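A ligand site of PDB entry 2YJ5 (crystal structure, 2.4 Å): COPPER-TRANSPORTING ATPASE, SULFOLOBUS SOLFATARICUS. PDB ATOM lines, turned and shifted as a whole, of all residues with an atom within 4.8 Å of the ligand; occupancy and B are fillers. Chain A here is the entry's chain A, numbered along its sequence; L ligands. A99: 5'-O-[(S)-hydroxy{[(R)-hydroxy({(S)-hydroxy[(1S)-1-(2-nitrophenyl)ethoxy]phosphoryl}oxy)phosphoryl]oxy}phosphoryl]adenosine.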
ATOM      1  N   THR A  36      23.756  22.786 -10.643  1.00  0.00           N
ATOM      2  CA  THR A  36      23.355  21.701  -9.772  1.00  0.00           C
ATOM      3  C   THR A  36      22.880  22.210  -8.420  1.00  0.00           C
ATOM      4  O   THR A  36      23.562  22.974  -7.743  1.00  0.00           O
ATOM      5  CB  THR A  36      24.511  20.662  -9.604  1.00  0.00           C
ATOM      6  OG1 THR A  36      25.011  20.282 -10.899  1.00  0.00           O
ATOM      7  CG2 THR A  36      24.017  19.419  -8.878  1.00  0.00           C
ATOM      8  N   GLY A  42      19.227  18.554  -7.333  1.00  0.00           N
ATOM      9  CA  GLY A  42      20.469  17.884  -6.982  1.00  0.00           C
ATOM     10  C   GLY A  42      20.249  16.415  -6.606  1.00  0.00           C
ATOM     11  O   GLY A  42      20.809  15.929  -5.624  1.00  0.00           O
ATOM     12  N   THR A  43      19.444  15.706  -7.391  1.00  0.00           N
ATOM     13  CA  THR A  43      18.984  14.386  -6.990  1.00  0.00           C
ATOM     14  C   THR A  43      18.932  13.378  -8.164  1.00  0.00           C
ATOM     15  O   THR A  43      17.981  13.384  -8.960  1.00  0.00           O
ATOM     16  CB  THR A  43      17.609  14.479  -6.282  1.00  0.00           C
ATOM     17  OG1 THR A  43      17.306  13.230  -5.652  1.00  0.00           O
ATOM     18  CG2 THR A  43      16.496  14.854  -7.272  1.00  0.00           C
ATOM     19  N   PRO A  44      19.943  12.505  -8.268  1.00  0.00           N
ATOM     20  CA  PRO A  44      20.022  11.582  -9.426  1.00  0.00           C
ATOM     21  C   PRO A  44      18.839  10.613  -9.523  1.00  0.00           C
ATOM     22  O   PRO A  44      18.354  10.116  -8.500  1.00  0.00           O
ATOM     23  CB  PRO A  44      21.319  10.825  -9.175  1.00  0.00           C
ATOM     24  CG  PRO A  44      21.576  10.950  -7.686  1.00  0.00           C
ATOM     25  CD  PRO A  44      21.058  12.325  -7.328  1.00  0.00           C
ATOM     26  N   GLU A  63      24.193  -3.078  -5.370  1.00  0.00           N
ATOM     27  CA  GLU A  63      24.120  -1.643  -5.038  1.00  0.00           C
ATOM     28  C   GLU A  63      23.295  -1.435  -3.770  1.00  0.00           C
ATOM     29  O   GLU A  63      23.361  -0.363  -3.159  1.00  0.00           O
ATOM     30  CB  GLU A  63      23.499  -0.814  -6.191  1.00  0.00           C
ATOM     31  CG  GLU A  63      24.351  -0.671  -7.469  1.00  0.00           C
ATOM     32  CD  GLU A  63      25.438   0.412  -7.374  1.00  0.00           C
ATOM     33  OE1 GLU A  63      25.834   0.781  -6.254  1.00  0.00           O
ATOM     34  OE2 GLU A  63      25.921   0.891  -8.424  1.00  0.00           O
ATOM     35  N   SER A  66      25.441  -0.405  -0.747  1.00  0.00           N
ATOM     36  CA  SER A  66      26.034   0.935  -0.709  1.00  0.00           C
ATOM     37  C   SER A  66      25.019   1.975  -0.248  1.00  0.00           C
ATOM     38  O   SER A  66      23.810   1.725  -0.259  1.00  0.00           O
ATOM     39  CB  SER A  66      26.612   1.310  -2.079  1.00  0.00           C
ATOM     40  OG  SER A  66      27.148   2.628  -2.069  1.00  0.00           O
ATOM     41  N   HIS A  68      25.822   5.410  -1.279  1.00  0.00           N
ATOM     42  CA  HIS A  68      26.068   6.441  -2.285  1.00  0.00           C
ATOM     43  C   HIS A  68      24.765   6.733  -3.057  1.00  0.00           C
ATOM     44  O   HIS A  68      24.044   5.809  -3.436  1.00  0.00           O
ATOM     45  CB  HIS A  68      27.197   5.943  -3.214  1.00  0.00           C
ATOM     46  CG  HIS A  68      27.618   6.918  -4.275  1.00  0.00           C
ATOM     47  ND1 HIS A  68      26.717   7.672  -5.002  1.00  0.00           N
ATOM     48  CD2 HIS A  68      28.849   7.235  -4.741  1.00  0.00           C
ATOM     49  CE1 HIS A  68      27.387   8.426  -5.863  1.00  0.00           C
ATOM     50  NE2 HIS A  68      28.676   8.181  -5.726  1.00  0.00           N
ATOM     51  N   ILE A  70      24.067   7.407  -6.096  1.00  0.00           N
ATOM     52  CA  ILE A  70      23.945   6.639  -7.335  1.00  0.00           C
ATOM     53  C   ILE A  70      23.398   5.217  -7.062  1.00  0.00           C
ATOM     54  O   ILE A  70      22.511   4.724  -7.748  1.00  0.00           O
ATOM     55  CB  ILE A  70      25.265   6.568  -8.093  1.00  0.00           C
ATOM     56  CG1 ILE A  70      25.546   7.892  -8.800  1.00  0.00           C
ATOM     57  CG2 ILE A  70      25.269   5.438  -9.093  1.00  0.00           C
ATOM     58  CD1 ILE A  70      26.951   7.980  -9.377  1.00  0.00           C
ATOM     59  N   ALA A  71      23.912   4.575  -6.023  1.00  0.00           N
ATOM     60  CA  ALA A  71      23.437   3.246  -5.691  1.00  0.00           C
ATOM     61  C   ALA A  71      21.972   3.294  -5.279  1.00  0.00           C
ATOM     62  O   ALA A  71      21.169   2.461  -5.703  1.00  0.00           O
ATOM     63  CB  ALA A  71      24.285   2.625  -4.602  1.00  0.00           C
ATOM     64  N   GLU A  93      33.211  -2.154  -1.536  1.00  0.00           N
ATOM     65  CA  GLU A  93      33.039  -0.829  -2.119  1.00  0.00           C
ATOM     66  C   GLU A  93      34.396  -0.145  -2.253  1.00  0.00           C
ATOM     67  O   GLU A  93      35.265  -0.315  -1.405  1.00  0.00           O
ATOM     68  CB  GLU A  93      32.091   0.030  -1.286  1.00  0.00           C
ATOM     69  CG  GLU A  93      31.856   1.388  -1.886  1.00  0.00           C
ATOM     70  CD  GLU A  93      30.633   2.067  -1.340  1.00  0.00           C
ATOM     71  OE1 GLU A  93      30.359   1.950  -0.121  1.00  0.00           O
ATOM     72  OE2 GLU A  93      29.920   2.724  -2.150  1.00  0.00           O
ATOM     73  N   GLY A  96      35.231   6.437  -5.441  1.00  0.00           N
ATOM     74  CA  GLY A  96      35.726   7.018  -6.676  1.00  0.00           C
ATOM     75  C   GLY A  96      35.502   6.132  -7.889  1.00  0.00           C
ATOM     76  O   GLY A  96      35.563   6.607  -9.037  1.00  0.00           O
ATOM     77  N   ILE A  97      35.222   4.851  -7.646  1.00  0.00           N
ATOM     78  CA  ILE A  97      35.100   3.859  -8.719  1.00  0.00           C
ATOM     79  C   ILE A  97      33.709   3.208  -8.736  1.00  0.00           C
ATOM     80  O   ILE A  97      32.915   3.435  -9.649  1.00  0.00           O
ATOM     81  CB  ILE A  97      36.189   2.764  -8.589  1.00  0.00           C
ATOM     82  CG1 ILE A  97      37.574   3.366  -8.779  1.00  0.00           C
ATOM     83  CG2 ILE A  97      35.968   1.646  -9.591  1.00  0.00           C
ATOM     84  CD1 ILE A  97      38.706   2.356  -8.698  1.00  0.00           C
ATOM     85  N   GLY A  98      33.425   2.403  -7.726  1.00  0.00           N
ATOM     86  CA  GLY A  98      32.128   1.806  -7.595  1.00  0.00           C
ATOM     87  C   GLY A  98      32.116   0.581  -6.699  1.00  0.00           C
ATOM     88  O   GLY A  98      32.720   0.570  -5.622  1.00  0.00           O
ATOM     89  N   VAL A  99      31.465  -0.471  -7.173  1.00  0.00           N
ATOM     90  CA  VAL A  99      31.007  -1.528  -6.297  1.00  0.00           C
ATOM     91  C   VAL A  99      31.253  -2.907  -6.911  1.00  0.00           C
ATOM     92  O   VAL A  99      31.314  -3.048  -8.125  1.00  0.00           O
ATOM     93  CB  VAL A  99      29.524  -1.264  -5.943  1.00  0.00           C
ATOM     94  CG1 VAL A  99      28.752  -2.510  -5.867  1.00  0.00           C
ATOM     95  CG2 VAL A  99      29.433  -0.468  -4.649  1.00  0.00           C
ATOM     96  N   VAL A 110      29.739  -2.972 -10.844  1.00  0.00           N
ATOM     97  CA  VAL A 110      29.005  -1.819 -11.328  1.00  0.00           C
ATOM     98  C   VAL A 110      29.889  -0.569 -11.206  1.00  0.00           C
ATOM     99  O   VAL A 110      30.266  -0.171 -10.097  1.00  0.00           O
ATOM    100  CB  VAL A 110      27.734  -1.602 -10.516  1.00  0.00           C
ATOM    101  CG1 VAL A 110      26.942  -0.460 -11.129  1.00  0.00           C
ATOM    102  CG2 VAL A 110      26.929  -2.915 -10.433  1.00  0.00           C
ATOM    103  N   LYS A 111      30.189   0.051 -12.340  1.00  0.00           N
ATOM    104  CA  LYS A 111      31.102   1.188 -12.378  1.00  0.00           C
ATOM    105  C   LYS A 111      30.937   2.044 -13.630  1.00  0.00           C
ATOM    106  O   LYS A 111      30.206   1.682 -14.565  1.00  0.00           O
ATOM    107  CB  LYS A 111      32.553   0.695 -12.276  1.00  0.00           C
ATOM    108  CG  LYS A 111      32.964  -0.252 -13.394  1.00  0.00           C
ATOM    109  CD  LYS A 111      34.408  -0.710 -13.210  1.00  0.00           C
ATOM    110  CE  LYS A 111      34.765  -1.813 -14.201  1.00  0.00           C
ATOM    111  NZ  LYS A 111      36.044  -2.543 -13.862  1.00  0.00           N
ATOM    112  N   LYS A 112      31.629   3.170 -13.644  1.00  0.00           N
ATOM    113  CA  LYS A 112      31.675   4.079 -14.783  1.00  0.00           C
ATOM    114  C   LYS A 112      32.028   3.322 -16.059  1.00  0.00           C
ATOM    115  O   LYS A 112      32.951   2.496 -16.073  1.00  0.00           O
ATOM    116  CB  LYS A 112      32.705   5.194 -14.531  1.00  0.00           C
ATOM    117  CG  LYS A 112      33.307   5.219 -13.075  1.00  0.00           C
ATOM    118  CD  LYS A 112      34.092   3.931 -12.644  1.00  0.00           C
ATOM    119  CE  LYS A 112      35.043   3.459 -13.763  1.00  0.00           C
ATOM    120  NZ  LYS A 112      36.089   2.465 -13.376  1.00  0.00           N
ATOM    121  N   ILE A 119      26.770   4.563 -16.653  1.00  0.00           N
ATOM    122  CA  ILE A 119      27.137   3.521 -15.677  1.00  0.00           C
ATOM    123  C   ILE A 119      26.986   2.127 -16.274  1.00  0.00           C
ATOM    124  O   ILE A 119      25.928   1.795 -16.832  1.00  0.00           O
ATOM    125  CB  ILE A 119      26.306   3.594 -14.373  1.00  0.00           C
ATOM    126  CG1 ILE A 119      26.307   5.020 -13.792  1.00  0.00           C
ATOM    127  CG2 ILE A 119      26.817   2.558 -13.356  1.00  0.00           C
ATOM    128  CD1 ILE A 119      27.497   5.324 -12.925  1.00  0.00           C
ATOM    129  N   ILE A 133      22.133   8.200 -16.171  1.00  0.00           N
ATOM    130  CA  ILE A 133      21.665   8.849 -14.945  1.00  0.00           C
ATOM    131  C   ILE A 133      21.641  10.403 -15.015  1.00  0.00           C
ATOM    132  O   ILE A 133      22.641  11.029 -15.368  1.00  0.00           O
ATOM    133  CB  ILE A 133      22.472   8.299 -13.736  1.00  0.00           C
ATOM    134  CG1 ILE A 133      21.828   6.959 -13.290  1.00  0.00           C
ATOM    135  CG2 ILE A 133      22.591   9.348 -12.610  1.00  0.00           C
ATOM    136  CD1 ILE A 133      22.293   6.376 -11.960  1.00  0.00           C
ATOM    137  N   SER A 134      20.489  11.009 -14.689  1.00  0.00           N
ATOM    138  CA  SER A 134      20.306  12.473 -14.728  1.00  0.00           C
ATOM    139  C   SER A 134      19.784  13.081 -13.416  1.00  0.00           C
ATOM    140  O   SER A 134      19.352  12.374 -12.517  1.00  0.00           O
ATOM    141  CB  SER A 134      19.349  12.896 -15.858  1.00  0.00           C
ATOM    142  OG  SER A 134      19.879  12.580 -17.136  1.00  0.00           O
ATOM    143  N   ASP A 135      19.808  14.420 -13.340  1.00  0.00           N
ATOM    144  CA  ASP A 135      19.303  15.177 -12.193  1.00  0.00           C
ATOM    145  C   ASP A 135      17.830  15.529 -12.427  1.00  0.00           C
ATOM    146  O   ASP A 135      17.313  15.299 -13.512  1.00  0.00           O
ATOM    147  CB  ASP A 135      20.145  16.438 -12.012  1.00  0.00           C
ATOM    148  CG  ASP A 135      20.057  17.024 -10.612  1.00  0.00           C
ATOM    149  OD1 ASP A 135      19.004  16.871  -9.948  1.00  0.00           O
ATOM    150  OD2 ASP A 135      21.059  17.633 -10.166  1.00  0.00           O
HETATM  151  C'  A99 L   1      25.597  12.371  -8.007  1.00  0.00           C
HETATM  152  N1  A99 L   1      27.871   2.657  -8.366  1.00  0.00           N
HETATM  153  C2  A99 L   1      28.189   2.895  -9.655  1.00  0.00           C
HETATM  154  N3  A99 L   1      29.118   3.794 -10.037  1.00  0.00           N
HETATM  155  C4  A99 L   1      29.810   4.530  -9.126  1.00  0.00           C
HETATM  156  C5  A99 L   1      29.495   4.333  -7.694  1.00  0.00           C
HETATM  157  C6  A99 L   1      28.457   3.313  -7.338  1.00  0.00           C
HETATM  158  N6  A99 L   1      28.105   3.034  -6.058  1.00  0.00           N
HETATM  159  N7  A99 L   1      30.307   5.182  -7.035  1.00  0.00           N
HETATM  160  C8  A99 L   1      31.061   5.869  -7.956  1.00  0.00           C
HETATM  161  N9  A99 L   1      30.746   5.476  -9.202  1.00  0.00           N
HETATM  162  PA  A99 L   1      32.312   9.781  -7.154  1.00  0.00           P
HETATM  163  PB  A99 L   1      30.505  11.873  -7.470  1.00  0.00           P
HETATM  164  PG  A99 L   1      28.172  12.414  -8.880  1.00  0.00           P
HETATM  165  O'L A99 L   1      25.154  15.997  -7.446  1.00  0.00           O
HETATM  166  O'M A99 L   1      23.485  15.047  -6.582  1.00  0.00           O
HETATM  167  C1' A99 L   1      23.242  14.962  -9.721  1.00  0.00           C
HETATM  168  O1A A99 L   1      33.362  10.870  -7.234  1.00  0.00           O
HETATM  169  C1B A99 L   1      31.361   5.979 -10.476  1.00  0.00           C
HETATM  170  O1B A99 L   1      30.830  12.276  -6.044  1.00  0.00           O
HETATM  171  O1G A99 L   1      28.757  11.850 -10.163  1.00  0.00           O
HETATM  172  C2' A99 L   1      24.059  14.443  -8.722  1.00  0.00           C
HETATM  173  N2' A99 L   1      24.235  15.191  -7.533  1.00  0.00           N
HETATM  174  O2' A99 L   1      30.656   6.825 -12.572  1.00  0.00           O
HETATM  175  O2A A99 L   1      32.016   9.062  -5.853  1.00  0.00           O
HETATM  176  C2B A99 L   1      30.425   6.950 -11.154  1.00  0.00           C
HETATM  177  O2B A99 L   1      31.044  12.650  -8.661  1.00  0.00           O
HETATM  178  O2G A99 L   1      26.673  11.803  -8.765  1.00  0.00           O
HETATM  179  C3' A99 L   1      24.705  13.096  -8.972  1.00  0.00           C
HETATM  180  O3' A99 L   1      30.444   9.385 -11.383  1.00  0.00           O
HETATM  181  O3A A99 L   1      30.908  10.332  -7.686  1.00  0.00           O
HETATM  182  C3B A99 L   1      30.873   8.281 -10.593  1.00  0.00           C
HETATM  183  O3B A99 L   1      28.916  11.721  -7.644  1.00  0.00           O
HETATM  184  O3G A99 L   1      28.157  13.910  -8.641  1.00  0.00           O
HETATM  185  C4' A99 L   1      24.458  12.454 -10.183  1.00  0.00           C
HETATM  186  O4' A99 L   1      32.578   6.715 -10.235  1.00  0.00           O
HETATM  187  C4B A99 L   1      32.375   8.105 -10.569  1.00  0.00           C
HETATM  188  C5' A99 L   1      23.628  13.040 -11.138  1.00  0.00           C
HETATM  189  O5' A99 L   1      32.621   8.665  -8.277  1.00  0.00           O
HETATM  190  C5B A99 L   1      33.088   9.010  -9.575  1.00  0.00           C
HETATM  191  C6' A99 L   1      23.034  14.269 -10.912  1.00  0.00           C
HETATM  192  CM' A99 L   1      26.119  13.167  -6.811  1.00  0.00           C
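An oxygen (O'M) of the ligand sits close to the backbone carbonyl oxygen of Gly 42 (3.0 Å). An oxygen (O4') of the ligand sits close to the backbone carbonyl oxygen of Gly 96 (3.2 Å). O of Ile 97 sits close to N9 of the ligand (3.0 Å). Residues that only touch the ligand: Thr 36, Pro 44, Ile 70, Gly 98, Val 110, Lys 112, Ile 119 and Asp 135. Of the 21 residues printed, 13 come within 4 Å of the ligand.
The side-chain carboxylate of Asp 135 is in hydrogen-bond range of the backbone NH of Gly 42. ND1 of His 68 is in hydrogen-bond range of N of Ile 70. The backbone NH (N) of His 68 lies within hydrogen-bond range of the side-chain hydroxyl (OG) of Ser 66 (3.2 Å). The side-chain carboxylate of Asp 135 lies within hydrogen-bond range of the backbone NH of Thr 43 (2.8 Å). The backbone NH of Val 110 sits at hydrogen-bond distance from the backbone carbonyl oxygen of Val 99, 3.1 Å away.
A nitrogen (N1) of the ligand is in hydrogen-bond range of the side-chain carboxylate (OE2) of Glu 63 (2.6 Å). A ring nitrogen (NE2) of His 68 sits at hydrogen-bond distance from an oxygen (O2A) of the ligand (3.5 Å).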
